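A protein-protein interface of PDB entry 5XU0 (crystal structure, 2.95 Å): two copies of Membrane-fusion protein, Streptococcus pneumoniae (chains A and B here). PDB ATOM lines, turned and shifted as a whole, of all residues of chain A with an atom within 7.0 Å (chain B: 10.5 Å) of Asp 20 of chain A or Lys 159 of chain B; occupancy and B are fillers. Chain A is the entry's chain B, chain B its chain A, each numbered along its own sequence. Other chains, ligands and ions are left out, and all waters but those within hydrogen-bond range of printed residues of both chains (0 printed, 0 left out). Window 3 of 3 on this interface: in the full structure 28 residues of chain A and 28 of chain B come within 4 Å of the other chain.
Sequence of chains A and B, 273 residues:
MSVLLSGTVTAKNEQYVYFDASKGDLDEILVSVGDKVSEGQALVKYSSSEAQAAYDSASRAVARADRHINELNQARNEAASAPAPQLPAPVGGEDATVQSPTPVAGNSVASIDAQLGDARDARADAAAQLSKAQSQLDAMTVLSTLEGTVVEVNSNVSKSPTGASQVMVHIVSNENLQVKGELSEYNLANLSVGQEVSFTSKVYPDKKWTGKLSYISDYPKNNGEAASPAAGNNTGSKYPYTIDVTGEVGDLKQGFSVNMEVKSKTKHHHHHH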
ATOM      1  N   TYR A  18       8.843 -33.753 -24.373  1.00  0.00           N
ATOM      2  CA  TYR A  18       7.461 -33.990 -23.992  1.00  0.00           C
ATOM      3  C   TYR A  18       6.792 -34.861 -25.042  1.00  0.00           C
ATOM      4  O   TYR A  18       7.212 -34.898 -26.201  1.00  0.00           O
ATOM      5  CB  TYR A  18       6.682 -32.675 -23.861  1.00  0.00           C
ATOM      6  CG  TYR A  18       7.364 -31.574 -23.071  1.00  0.00           C
ATOM      7  CD1 TYR A  18       7.286 -31.534 -21.687  1.00  0.00           C
ATOM      8  CD2 TYR A  18       8.059 -30.556 -23.714  1.00  0.00           C
ATOM      9  CE1 TYR A  18       7.890 -30.519 -20.968  1.00  0.00           C
ATOM     10  CE2 TYR A  18       8.667 -29.537 -22.999  1.00  0.00           C
ATOM     11  CZ  TYR A  18       8.581 -29.524 -21.628  1.00  0.00           C
ATOM     12  OH  TYR A  18       9.185 -28.514 -20.907  1.00  0.00           O
ATOM     13  N   PHE A  19       5.737 -35.553 -24.629  1.00  0.00           N
ATOM     14  CA  PHE A  19       4.976 -36.376 -25.557  1.00  0.00           C
ATOM     15  C   PHE A  19       4.354 -35.514 -26.652  1.00  0.00           C
ATOM     16  O   PHE A  19       3.973 -34.361 -26.429  1.00  0.00           O
ATOM     17  CB  PHE A  19       3.888 -37.146 -24.809  1.00  0.00           C
ATOM     18  CG  PHE A  19       3.111 -38.093 -25.675  1.00  0.00           C
ATOM     19  CD1 PHE A  19       3.604 -39.355 -25.960  1.00  0.00           C
ATOM     20  CD2 PHE A  19       1.887 -37.721 -26.205  1.00  0.00           C
ATOM     21  CE1 PHE A  19       2.892 -40.228 -26.758  1.00  0.00           C
ATOM     22  CE2 PHE A  19       1.170 -38.590 -27.004  1.00  0.00           C
ATOM     23  CZ  PHE A  19       1.673 -39.846 -27.280  1.00  0.00           C
ATOM     24  N   ASP A  20       4.258 -36.087 -27.851  1.00  0.00           N
ATOM     25  CA  ASP A  20       3.675 -35.399 -29.002  1.00  0.00           C
ATOM     26  C   ASP A  20       2.741 -36.368 -29.712  1.00  0.00           C
ATOM     27  O   ASP A  20       3.201 -37.298 -30.383  1.00  0.00           O
ATOM     28  CB  ASP A  20       4.760 -34.889 -29.951  1.00  0.00           C
ATOM     29  CG  ASP A  20       4.223 -33.920 -30.990  1.00  0.00           C
ATOM     30  OD1 ASP A  20       2.986 -33.830 -31.150  1.00  0.00           O
ATOM     31  OD2 ASP A  20       5.043 -33.255 -31.655  1.00  0.00           O
ATOM     32  N   ALA A  21       1.432 -36.147 -29.565  1.00  0.00           N
ATOM     33  CA  ALA A  21       0.444 -37.001 -30.216  1.00  0.00           C
ATOM     34  C   ALA A  21       0.517 -36.900 -31.734  1.00  0.00           C
ATOM     35  O   ALA A  21       0.263 -37.888 -32.433  1.00  0.00           O
ATOM     36  CB  ALA A  21      -0.956 -36.633 -29.736  1.00  0.00           C
ATOM     37  N   SER A  22       0.860 -35.721 -32.259  1.00  0.00           N
ATOM     38  CA  SER A  22       0.961 -35.530 -33.701  1.00  0.00           C
ATOM     39  C   SER A  22       2.079 -36.351 -34.329  1.00  0.00           C
ATOM     40  O   SER A  22       2.161 -36.414 -35.560  1.00  0.00           O
ATOM     41  CB  SER A  22       1.162 -34.048 -34.017  1.00  0.00           C
ATOM     42  OG  SER A  22       2.528 -33.684 -33.910  1.00  0.00           O
ATOM     43  N   LYS A  23       2.942 -36.967 -33.523  1.00  0.00           N
ATOM     44  CA  LYS A  23       3.931 -37.905 -34.028  1.00  0.00           C
ATOM     45  C   LYS A  23       3.450 -39.348 -33.967  1.00  0.00           C
ATOM     46  O   LYS A  23       4.115 -40.228 -34.519  1.00  0.00           O
ATOM     47  CB  LYS A  23       5.247 -37.758 -33.253  1.00  0.00           C
ATOM     48  CG  LYS A  23       5.868 -36.371 -33.380  1.00  0.00           C
ATOM     49  CD  LYS A  23       7.369 -36.386 -33.131  1.00  0.00           C
ATOM     50  CE  LYS A  23       7.982 -35.021 -33.427  1.00  0.00           C
ATOM     51  NZ  LYS A  23       9.421 -35.107 -33.806  1.00  0.00           N
ATOM     52  N   GLY A  24       2.316 -39.610 -33.320  1.00  0.00           N
ATOM     53  CA  GLY A  24       1.710 -40.926 -33.382  1.00  0.00           C
ATOM     54  C   GLY A  24       1.665 -41.687 -32.073  1.00  0.00           C
ATOM     55  O   GLY A  24       0.930 -41.315 -31.152  1.00  0.00           O
ATOM     56  N   ASP A  25       2.439 -42.768 -31.989  1.00  0.00           N
ATOM     57  CA  ASP A  25       2.464 -43.646 -30.828  1.00  0.00           C
ATOM     58  C   ASP A  25       3.906 -43.925 -30.427  1.00  0.00           C
ATOM     59  O   ASP A  25       4.807 -43.944 -31.269  1.00  0.00           O
ATOM     60  CB  ASP A  25       1.743 -44.972 -31.112  1.00  0.00           C
ATOM     61  CG  ASP A  25       0.242 -44.804 -31.238  1.00  0.00           C
ATOM     62  OD1 ASP A  25      -0.307 -43.859 -30.632  1.00  0.00           O
ATOM     63  OD2 ASP A  25      -0.389 -45.617 -31.946  1.00  0.00           O
ATOM     64  N   TYR A  46       9.269 -43.162 -31.748  1.00  0.00           N
ATOM     65  CA  TYR A  46       7.879 -43.473 -32.023  1.00  0.00           C
ATOM     66  C   TYR A  46       7.795 -44.581 -33.072  1.00  0.00           C
ATOM     67  O   TYR A  46       8.751 -44.850 -33.804  1.00  0.00           O
ATOM     68  CB  TYR A  46       7.130 -42.230 -32.508  1.00  0.00           C
ATOM     69  CG  TYR A  46       7.006 -41.100 -31.504  1.00  0.00           C
ATOM     70  CD1 TYR A  46       5.894 -40.996 -30.675  1.00  0.00           C
ATOM     71  CD2 TYR A  46       7.985 -40.119 -31.406  1.00  0.00           C
ATOM     72  CE1 TYR A  46       5.770 -39.957 -29.764  1.00  0.00           C
ATOM     73  CE2 TYR A  46       7.871 -39.077 -30.501  1.00  0.00           C
ATOM     74  CZ  TYR A  46       6.761 -39.001 -29.683  1.00  0.00           C
ATOM     75  OH  TYR A  46       6.645 -37.965 -28.782  1.00  0.00           O
ATOM     76  N   SER A 165       1.594 -30.627 -19.596  1.00  0.00           N
ATOM     77  CA  SER A 165       2.607 -31.171 -20.491  1.00  0.00           C
ATOM     78  C   SER A 165       3.206 -32.428 -19.873  1.00  0.00           C
ATOM     79  O   SER A 165       3.549 -32.442 -18.687  1.00  0.00           O
ATOM     80  CB  SER A 165       3.700 -30.138 -20.763  1.00  0.00           C
ATOM     81  OG  SER A 165       3.140 -28.882 -21.110  1.00  0.00           O
ATOM     82  N   GLN A 166       3.329 -33.481 -20.679  1.00  0.00           N
ATOM     83  CA  GLN A 166       3.835 -34.769 -20.206  1.00  0.00           C
ATOM     84  C   GLN A 166       5.327 -34.852 -20.505  1.00  0.00           C
ATOM     85  O   GLN A 166       5.730 -35.163 -21.629  1.00  0.00           O
ATOM     86  CB  GLN A 166       3.072 -35.918 -20.858  1.00  0.00           C
ATOM     87  CG  GLN A 166       1.565 -35.856 -20.660  1.00  0.00           C
ATOM     88  CD  GLN A 166       0.982 -37.175 -20.186  1.00  0.00           C
ATOM     89  OE1 GLN A 166       0.352 -37.902 -20.953  1.00  0.00           O
ATOM     90  NE2 GLN A 166       1.194 -37.491 -18.913  1.00  0.00           N
ATOM     91  N   MET A 168       8.481 -36.597 -20.921  1.00  0.00           N
ATOM     92  CA  MET A 168       8.833 -37.993 -21.112  1.00  0.00           C
ATOM     93  C   MET A 168      10.302 -38.249 -20.816  1.00  0.00           C
ATOM     94  O   MET A 168      10.636 -39.269 -20.212  1.00  0.00           O
ATOM     95  CB  MET A 168       8.489 -38.452 -22.523  1.00  0.00           C
ATOM     96  CG  MET A 168       7.243 -39.319 -22.585  1.00  0.00           C
ATOM     97  SD  MET A 168       7.251 -40.467 -24.145  1.00  0.00           S
ATOM     98  CE  MET A 168       7.519 -39.083 -25.474  1.00  0.00           C
ATOM     99  N   TYR B  18       4.928 -16.297 -28.264  1.00  0.00           N
ATOM    100  CA  TYR B  18       4.489 -17.572 -27.721  1.00  0.00           C
ATOM    101  C   TYR B  18       4.610 -18.664 -28.775  1.00  0.00           C
ATOM    102  O   TYR B  18       4.622 -18.404 -29.981  1.00  0.00           O
ATOM    103  CB  TYR B  18       3.043 -17.485 -27.226  1.00  0.00           C
ATOM    104  CG  TYR B  18       2.773 -16.338 -26.278  1.00  0.00           C
ATOM    105  CD1 TYR B  18       2.464 -15.071 -26.758  1.00  0.00           C
ATOM    106  CD2 TYR B  18       2.815 -16.525 -24.903  1.00  0.00           C
ATOM    107  CE1 TYR B  18       2.211 -14.021 -25.895  1.00  0.00           C
ATOM    108  CE2 TYR B  18       2.563 -15.482 -24.033  1.00  0.00           C
ATOM    109  CZ  TYR B  18       2.263 -14.232 -24.533  1.00  0.00           C
ATOM    110  OH  TYR B  18       2.012 -13.188 -23.673  1.00  0.00           O
ATOM    111  N   PHE B  19       4.701 -19.903 -28.300  1.00  0.00           N
ATOM    112  CA  PHE B  19       4.709 -21.041 -29.208  1.00  0.00           C
ATOM    113  C   PHE B  19       3.359 -21.162 -29.901  1.00  0.00           C
ATOM    114  O   PHE B  19       2.311 -21.164 -29.248  1.00  0.00           O
ATOM    115  CB  PHE B  19       5.031 -22.326 -28.451  1.00  0.00           C
ATOM    116  CG  PHE B  19       5.009 -23.552 -29.315  1.00  0.00           C
ATOM    117  CD1 PHE B  19       5.896 -23.685 -30.372  1.00  0.00           C
ATOM    118  CD2 PHE B  19       4.097 -24.566 -29.079  1.00  0.00           C
ATOM    119  CE1 PHE B  19       5.876 -24.811 -31.174  1.00  0.00           C
ATOM    120  CE2 PHE B  19       4.073 -25.694 -29.878  1.00  0.00           C
ATOM    121  CZ  PHE B  19       4.964 -25.817 -30.927  1.00  0.00           C
ATOM    122  N   ASP B  20       3.384 -21.253 -31.226  1.00  0.00           N
ATOM    123  CA  ASP B  20       2.181 -21.411 -32.034  1.00  0.00           C
ATOM    124  C   ASP B  20       2.134 -22.848 -32.537  1.00  0.00           C
ATOM    125  O   ASP B  20       2.943 -23.241 -33.385  1.00  0.00           O
ATOM    126  CB  ASP B  20       2.165 -20.415 -33.191  1.00  0.00           C
ATOM    127  CG  ASP B  20       0.761 -20.095 -33.663  1.00  0.00           C
ATOM    128  OD1 ASP B  20      -0.115 -20.980 -33.571  1.00  0.00           O
ATOM    129  OD2 ASP B  20       0.537 -18.954 -34.119  1.00  0.00           O
ATOM    130  N   ALA B  21       1.193 -23.632 -32.002  1.00  0.00           N
ATOM    131  CA  ALA B  21       1.048 -25.014 -32.446  1.00  0.00           C
ATOM    132  C   ALA B  21       0.575 -25.079 -33.891  1.00  0.00           C
ATOM    133  O   ALA B  21       1.082 -25.887 -34.680  1.00  0.00           O
ATOM    134  CB  ALA B  21       0.079 -25.759 -31.529  1.00  0.00           C
ATOM    135  N   SER B  22      -0.384 -24.225 -34.259  1.00  0.00           N
ATOM    136  CA  SER B  22      -0.922 -24.207 -35.614  1.00  0.00           C
ATOM    137  C   SER B  22       0.132 -23.886 -36.667  1.00  0.00           C
ATOM    138  O   SER B  22      -0.147 -24.042 -37.861  1.00  0.00           O
ATOM    139  CB  SER B  22      -2.066 -23.197 -35.709  1.00  0.00           C
ATOM    140  OG  SER B  22      -1.577 -21.872 -35.839  1.00  0.00           O
ATOM    141  N   LYS B  23       1.321 -23.442 -36.263  1.00  0.00           N
ATOM    142  CA  LYS B  23       2.414 -23.194 -37.193  1.00  0.00           C
ATOM    143  C   LYS B  23       3.342 -24.392 -37.349  1.00  0.00           C
ATOM    144  O   LYS B  23       4.259 -24.342 -38.177  1.00  0.00           O
ATOM    145  CB  LYS B  23       3.216 -21.968 -36.751  1.00  0.00           C
ATOM    146  CG  LYS B  23       2.423 -20.668 -36.787  1.00  0.00           C
ATOM    147  CD  LYS B  23       3.334 -19.464 -36.981  1.00  0.00           C
ATOM    148  CE  LYS B  23       2.546 -18.164 -36.951  1.00  0.00           C
ATOM    149  NZ  LYS B  23       3.391 -16.995 -37.324  1.00  0.00           N
ATOM    150  N   GLY B  24       3.135 -25.460 -36.579  1.00  0.00           N
ATOM    151  CA  GLY B  24       3.855 -26.700 -36.806  1.00  0.00           C
ATOM    152  C   GLY B  24       4.888 -27.055 -35.756  1.00  0.00           C
ATOM    153  O   GLY B  24       4.542 -27.474 -34.647  1.00  0.00           O
ATOM    154  N   ASP B  25       6.164 -26.900 -36.104  1.00  0.00           N
ATOM    155  CA  ASP B  25       7.269 -27.289 -35.240  1.00  0.00           C
ATOM    156  C   ASP B  25       8.332 -26.202 -35.249  1.00  0.00           C
ATOM    157  O   ASP B  25       8.626 -25.619 -36.298  1.00  0.00           O
ATOM    158  CB  ASP B  25       7.891 -28.619 -35.692  1.00  0.00           C
ATOM    159  CG  ASP B  25       6.935 -29.787 -35.556  1.00  0.00           C
ATOM    160  OD1 ASP B  25       6.461 -30.044 -34.429  1.00  0.00           O
ATOM    161  OD2 ASP B  25       6.657 -30.452 -36.579  1.00  0.00           O
ATOM    162  N   LEU B  26       8.908 -25.937 -34.079  1.00  0.00           N
ATOM    163  CA  LEU B  26       9.993 -24.973 -33.958  1.00  0.00           C
ATOM    164  C   LEU B  26      11.288 -25.584 -34.484  1.00  0.00           C
ATOM    165  O   LEU B  26      11.642 -26.712 -34.128  1.00  0.00           O
ATOM    166  CB  LEU B  26      10.163 -24.550 -32.496  1.00  0.00           C
ATOM    167  CG  LEU B  26      11.329 -23.658 -32.024  1.00  0.00           C
ATOM    168  CD1 LEU B  26      11.812 -22.672 -33.083  1.00  0.00           C
ATOM    169  CD2 LEU B  26      10.926 -22.887 -30.794  1.00  0.00           C
ATOM    170  N   ASP B  27      11.990 -24.836 -35.336  1.00  0.00           N
ATOM    171  CA  ASP B  27      13.356 -25.195 -35.734  1.00  0.00           C
ATOM    172  C   ASP B  27      14.334 -24.704 -34.676  1.00  0.00           C
ATOM    173  O   ASP B  27      14.863 -25.500 -33.886  1.00  0.00           O
ATOM    174  CB  ASP B  27      13.673 -24.617 -37.116  1.00  0.00           C
ATOM    175  CG  ASP B  27      15.067 -24.977 -37.594  1.00  0.00           C
ATOM    176  OD1 ASP B  27      15.577 -26.049 -37.206  1.00  0.00           O
ATOM    177  OD2 ASP B  27      15.656 -24.183 -38.361  1.00  0.00           O
ATOM    178  N   TYR B  46      10.148 -21.336 -37.402  1.00  0.00           N
ATOM    179  CA  TYR B  46       9.488 -22.629 -37.423  1.00  0.00           C
ATOM    180  C   TYR B  46       9.969 -23.432 -38.631  1.00  0.00           C
ATOM    181  O   TYR B  46      10.599 -22.904 -39.551  1.00  0.00           O
ATOM    182  CB  TYR B  46       7.968 -22.466 -37.461  1.00  0.00           C
ATOM    183  CG  TYR B  46       7.356 -21.863 -36.210  1.00  0.00           C
ATOM    184  CD1 TYR B  46       6.744 -22.666 -35.255  1.00  0.00           C
ATOM    185  CD2 TYR B  46       7.378 -20.490 -35.993  1.00  0.00           C
ATOM    186  CE1 TYR B  46       6.179 -22.119 -34.114  1.00  0.00           C
ATOM    187  CE2 TYR B  46       6.816 -19.935 -34.854  1.00  0.00           C
ATOM    188  CZ  TYR B  46       6.218 -20.754 -33.920  1.00  0.00           C
ATOM    189  OH  TYR B  46       5.658 -20.204 -32.789  1.00  0.00           O
ATOM    190  N   SER B  47       9.675 -24.732 -38.619  1.00  0.00           N
ATOM    191  CA  SER B  47      10.012 -25.577 -39.757  1.00  0.00           C
ATOM    192  C   SER B  47       9.239 -25.115 -40.987  1.00  0.00           C
ATOM    193  O   SER B  47       8.004 -25.113 -40.989  1.00  0.00           O
ATOM    194  CB  SER B  47       9.701 -27.038 -39.440  1.00  0.00           C
ATOM    195  OG  SER B  47      10.397 -27.906 -40.318  1.00  0.00           O
ATOM    196  N   GLU B  50       7.181 -27.620 -45.163  1.00  0.00           N
ATOM    197  CA  GLU B  50       5.812 -27.817 -45.630  1.00  0.00           C
ATOM    198  C   GLU B  50       5.258 -26.541 -46.249  1.00  0.00           C
ATOM    199  O   GLU B  50       4.488 -26.592 -47.216  1.00  0.00           O
ATOM    200  CB  GLU B  50       4.924 -28.288 -44.478  1.00  0.00           C
ATOM    201  CG  GLU B  50       4.994 -29.783 -44.210  1.00  0.00           C
ATOM    202  CD  GLU B  50       3.625 -30.403 -44.009  1.00  0.00           C
ATOM    203  OE1 GLU B  50       2.733 -30.163 -44.851  1.00  0.00           O
ATOM    204  OE2 GLU B  50       3.439 -31.129 -43.009  1.00  0.00           O
ATOM    205  N   SER B 155      13.507 -22.513 -25.168  1.00  0.00           N
ATOM    206  CA  SER B 155      13.466 -23.459 -26.275  1.00  0.00           C
ATOM    207  C   SER B 155      12.816 -24.786 -25.904  1.00  0.00           C
ATOM    208  O   SER B 155      12.731 -25.673 -26.761  1.00  0.00           O
ATOM    209  CB  SER B 155      14.882 -23.720 -26.798  1.00  0.00           C
ATOM    210  OG  SER B 155      15.585 -22.508 -27.007  1.00  0.00           O
ATOM    211  N   ASN B 156      12.359 -24.948 -24.665  1.00  0.00           N
ATOM    212  CA  ASN B 156      11.816 -26.216 -24.184  1.00  0.00           C
ATOM    213  C   ASN B 156      10.328 -26.029 -23.896  1.00  0.00           C
ATOM    214  O   ASN B 156       9.898 -25.924 -22.747  1.00  0.00           O
ATOM    215  CB  ASN B 156      12.585 -26.698 -22.950  1.00  0.00           C
ATOM    216  CG  ASN B 156      13.872 -27.417 -23.314  1.00  0.00           C
ATOM    217  OD1 ASN B 156      13.907 -28.645 -23.408  1.00  0.00           O
ATOM    218  ND2 ASN B 156      14.937 -26.652 -23.531  1.00  0.00           N
ATOM    219  N   VAL B 157       9.536 -25.994 -24.968  1.00  0.00           N
ATOM    220  CA  VAL B 157       8.089 -25.864 -24.888  1.00  0.00           C
ATOM    221  C   VAL B 157       7.455 -27.006 -25.670  1.00  0.00           C
ATOM    222  O   VAL B 157       8.064 -27.566 -26.587  1.00  0.00           O
ATOM    223  CB  VAL B 157       7.610 -24.495 -25.420  1.00  0.00           C
ATOM    224  CG1 VAL B 157       8.235 -23.364 -24.611  1.00  0.00           C
ATOM    225  CG2 VAL B 157       7.946 -24.353 -26.900  1.00  0.00           C
ATOM    226  N   SER B 158       6.222 -27.352 -25.302  1.00  0.00           N
ATOM    227  CA  SER B 158       5.529 -28.507 -25.857  1.00  0.00           C
ATOM    228  C   SER B 158       4.336 -28.085 -26.706  1.00  0.00           C
ATOM    229  O   SER B 158       3.736 -27.031 -26.487  1.00  0.00           O
ATOM    230  CB  SER B 158       5.049 -29.442 -24.744  1.00  0.00           C
ATOM    231  OG  SER B 158       3.854 -28.961 -24.154  1.00  0.00           O
ATOM    232  N   LYS B 159       3.983 -28.934 -27.674  1.00  0.00           N
ATOM    233  CA  LYS B 159       2.766 -28.732 -28.460  1.00  0.00           C
ATOM    234  C   LYS B 159       1.646 -29.544 -27.818  1.00  0.00           C
ATOM    235  O   LYS B 159       1.349 -30.681 -28.192  1.00  0.00           O
ATOM    236  CB  LYS B 159       2.979 -29.108 -29.921  1.00  0.00           C
ATOM    237  CG  LYS B 159       3.814 -30.350 -30.149  1.00  0.00           C
ATOM    238  CD  LYS B 159       4.335 -30.388 -31.575  1.00  0.00           C
ATOM    239  CE  LYS B 159       3.230 -30.749 -32.554  1.00  0.00           C
ATOM    240  NZ  LYS B 159       3.765 -30.989 -33.921  1.00  0.00           N
ATOM    241  N   SER B 160       1.023 -28.935 -26.807  1.00  0.00           N
ATOM    242  CA  SER B 160      -0.142 -29.499 -26.150  1.00  0.00           C
ATOM    243  C   SER B 160      -0.860 -28.352 -25.468  1.00  0.00           C
ATOM    244  O   SER B 160      -0.189 -27.462 -24.927  1.00  0.00           O
ATOM    245  CB  SER B 160       0.237 -30.572 -25.122  1.00  0.00           C
ATOM    246  OG  SER B 160       0.544 -29.989 -23.867  1.00  0.00           O
ATOM    247  N   PRO B 161      -2.195 -28.313 -25.494  1.00  0.00           N
ATOM    248  CA  PRO B 161      -2.914 -27.327 -24.676  1.00  0.00           C
ATOM    249  C   PRO B 161      -2.488 -27.424 -23.220  1.00  0.00           C
ATOM    250  O   PRO B 161      -3.208 -27.967 -22.374  1.00  0.00           O
ATOM    251  CB  PRO B 161      -4.385 -27.710 -24.878  1.00  0.00           C
ATOM    252  CG  PRO B 161      -4.411 -28.357 -26.225  1.00  0.00           C
ATOM    253  CD  PRO B 161      -3.102 -29.091 -26.353  1.00  0.00           C
ATOM    254  N   THR B 162      -1.302 -26.888 -22.931  1.00  0.00           N
ATOM    255  CA  THR B 162      -0.601 -27.084 -21.668  1.00  0.00           C
ATOM    256  C   THR B 162      -1.276 -26.409 -20.485  1.00  0.00           C
ATOM    257  O   THR B 162      -0.709 -26.432 -19.386  1.00  0.00           O
ATOM    258  CB  THR B 162       0.836 -26.574 -21.802  1.00  0.00           C
ATOM    259  OG1 THR B 162       1.440 -26.480 -20.506  1.00  0.00           O
ATOM    260  CG2 THR B 162       0.853 -25.208 -22.474  1.00  0.00           C
ATOM    261  N   GLY B 163      -2.456 -25.818 -20.667  1.00  0.00           N
ATOM    262  CA  GLY B 163      -3.118 -25.085 -19.613  1.00  0.00           C
ATOM    263  C   GLY B 163      -2.606 -23.681 -19.393  1.00  0.00           C
ATOM    264  O   GLY B 163      -3.301 -22.876 -18.762  1.00  0.00           O
ATOM    265  N   ALA B 164      -1.410 -23.360 -19.885  1.00  0.00           N
ATOM    266  CA  ALA B 164      -0.874 -22.007 -19.810  1.00  0.00           C
ATOM    267  C   ALA B 164      -0.357 -21.576 -21.177  1.00  0.00           C
ATOM    268  O   ALA B 164      -0.514 -22.303 -22.163  1.00  0.00           O
ATOM    269  CB  ALA B 164       0.235 -21.923 -18.759  1.00  0.00           C
ATOM    270  N   GLN B 166       2.962 -20.601 -23.340  1.00  0.00           N
ATOM    271  CA  GLN B 166       4.399 -20.868 -23.287  1.00  0.00           C
ATOM    272  C   GLN B 166       5.151 -19.737 -23.975  1.00  0.00           C
ATOM    273  O   GLN B 166       5.248 -19.691 -25.203  1.00  0.00           O
ATOM    274  CB  GLN B 166       4.710 -22.216 -23.923  1.00  0.00           C
ATOM    275  CG  GLN B 166       3.780 -23.320 -23.463  1.00  0.00           C
ATOM    276  CD  GLN B 166       4.339 -24.695 -23.738  1.00  0.00           C
ATOM    277  OE1 GLN B 166       4.513 -25.082 -24.888  1.00  0.00           O
ATOM    278  NE2 GLN B 166       4.626 -25.443 -22.678  1.00  0.00           N
ATOM    279  N   MET B 168       8.207 -17.824 -25.454  1.00  0.00           N
ATOM    280  CA  MET B 168       9.399 -18.319 -26.134  1.00  0.00           C
ATOM    281  C   MET B 168      10.472 -17.247 -26.225  1.00  0.00           C
ATOM    282  O   MET B 168      11.656 -17.529 -26.061  1.00  0.00           O
ATOM    283  CB  MET B 168       9.052 -18.822 -27.535  1.00  0.00           C
ATOM    284  CG  MET B 168       8.445 -20.210 -27.567  1.00  0.00           C
ATOM    285  SD  MET B 168       8.563 -20.985 -29.349  1.00  0.00           S
ATOM    286  CE  MET B 168       8.383 -19.343 -30.379  1.00  0.00           C
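The backbone carbonyl oxygen (O) of Asn 156 of chain B lies within hydrogen-bond range of the side-chain hydroxyl (OH) of Tyr 18 of chain A (3.3 Å).
OG of Ser 165 of chain A is in hydrogen-bond range of OG of Ser 158 of chain B, at 3.1 Å.
OD2 of Asp 20 of chain A lies within salt-bridge range of NZ of Lys 159 of chain B, 3.5 Å away.
The side-chain amino group of Lys 159 of chain B lies within hydrogen-bond range of the side-chain hydroxyl of Ser 22 of chain A.
The side-chain hydroxyl (OG) of Ser 165 of chain A lies within hydrogen-bond range of the side-chain hydroxyl (OG1) of Thr 162 of chain B.
The side-chain carboxylate (OD1) of Asp 25 of chain B lies within salt-bridge range of the side-chain amino group (NZ) of Lys 159 of chain B.
OG of Ser 158 of chain B is in hydrogen-bond range of OG of Ser 160 of chain B (3.5 Å).
O of Ser 158 of chain B lies close to OE1 of Gln 166 of chain B (2.6 Å).
The side-chain hydroxyl (OG) of Ser 22 of chain A sits at hydrogen-bond distance from the side-chain carboxylate (OD1) of Asp 20 of chain A.
OH of Tyr 46 of chain A lies within hydrogen-bond range of N of Asp 20 of chain A (3.2 Å).
Among the printed residues, merely in contact across the chains: Tyr 18 of chain A with Val 157 of chain B, Tyr 18 of chain A with Ser 158 of chain B and Ser 165 of chain A with Ser 160 of chain B.
No residue of chain B comes within 4 Å of Phe 19 of chain A.
No residue of chain B comes within 4 Å of Ala 21 of chain A.
Of chain B, only Lys 159 comes within 4 Å of Ser 22 of chain A.
No residue of chain B comes within 4 Å of Lys 23 of chain A.
No residue of chain B comes within 4 Å of Gly 24 of chain A.
Of the printed residues of chain A, Thr 162 of chain B touches Ser 165 (3.0 Å).
Of the printed residues of chain A, Val 157 of chain B touches Tyr 18 (3.9 Å).
Printed residues of chain B within 4 Å of Ser 165 of chain A: Ser 158, Ser 160 and Thr 162.
Printed residues of chain A within 4 Å of Ser 158 of chain B: Tyr 18 and Ser 165.
Printed residues of chain A within 4 Å of Asn 156 of chain B: Tyr 18.
Gly 24 of chain B touches none of the printed residues of chain A.
Of the 12 printed residues of chain A, 4 touch a printed residue of chain B.
Among the printed residues, Asp or Glu carboxylates within 4 Å of a Lys or Arg side-chain nitrogen of the other chain: Asp 20 of chain A with Lys 159 of chain B (3.5 Å).
Positions printed for both chains: 18, 19, 20, 21, 22, 23, 24, 25, 46, 166 and 168.
Of the 8 pairs that touch across the chains among the printed residues, none has its exchanged pair printed and touching as well.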
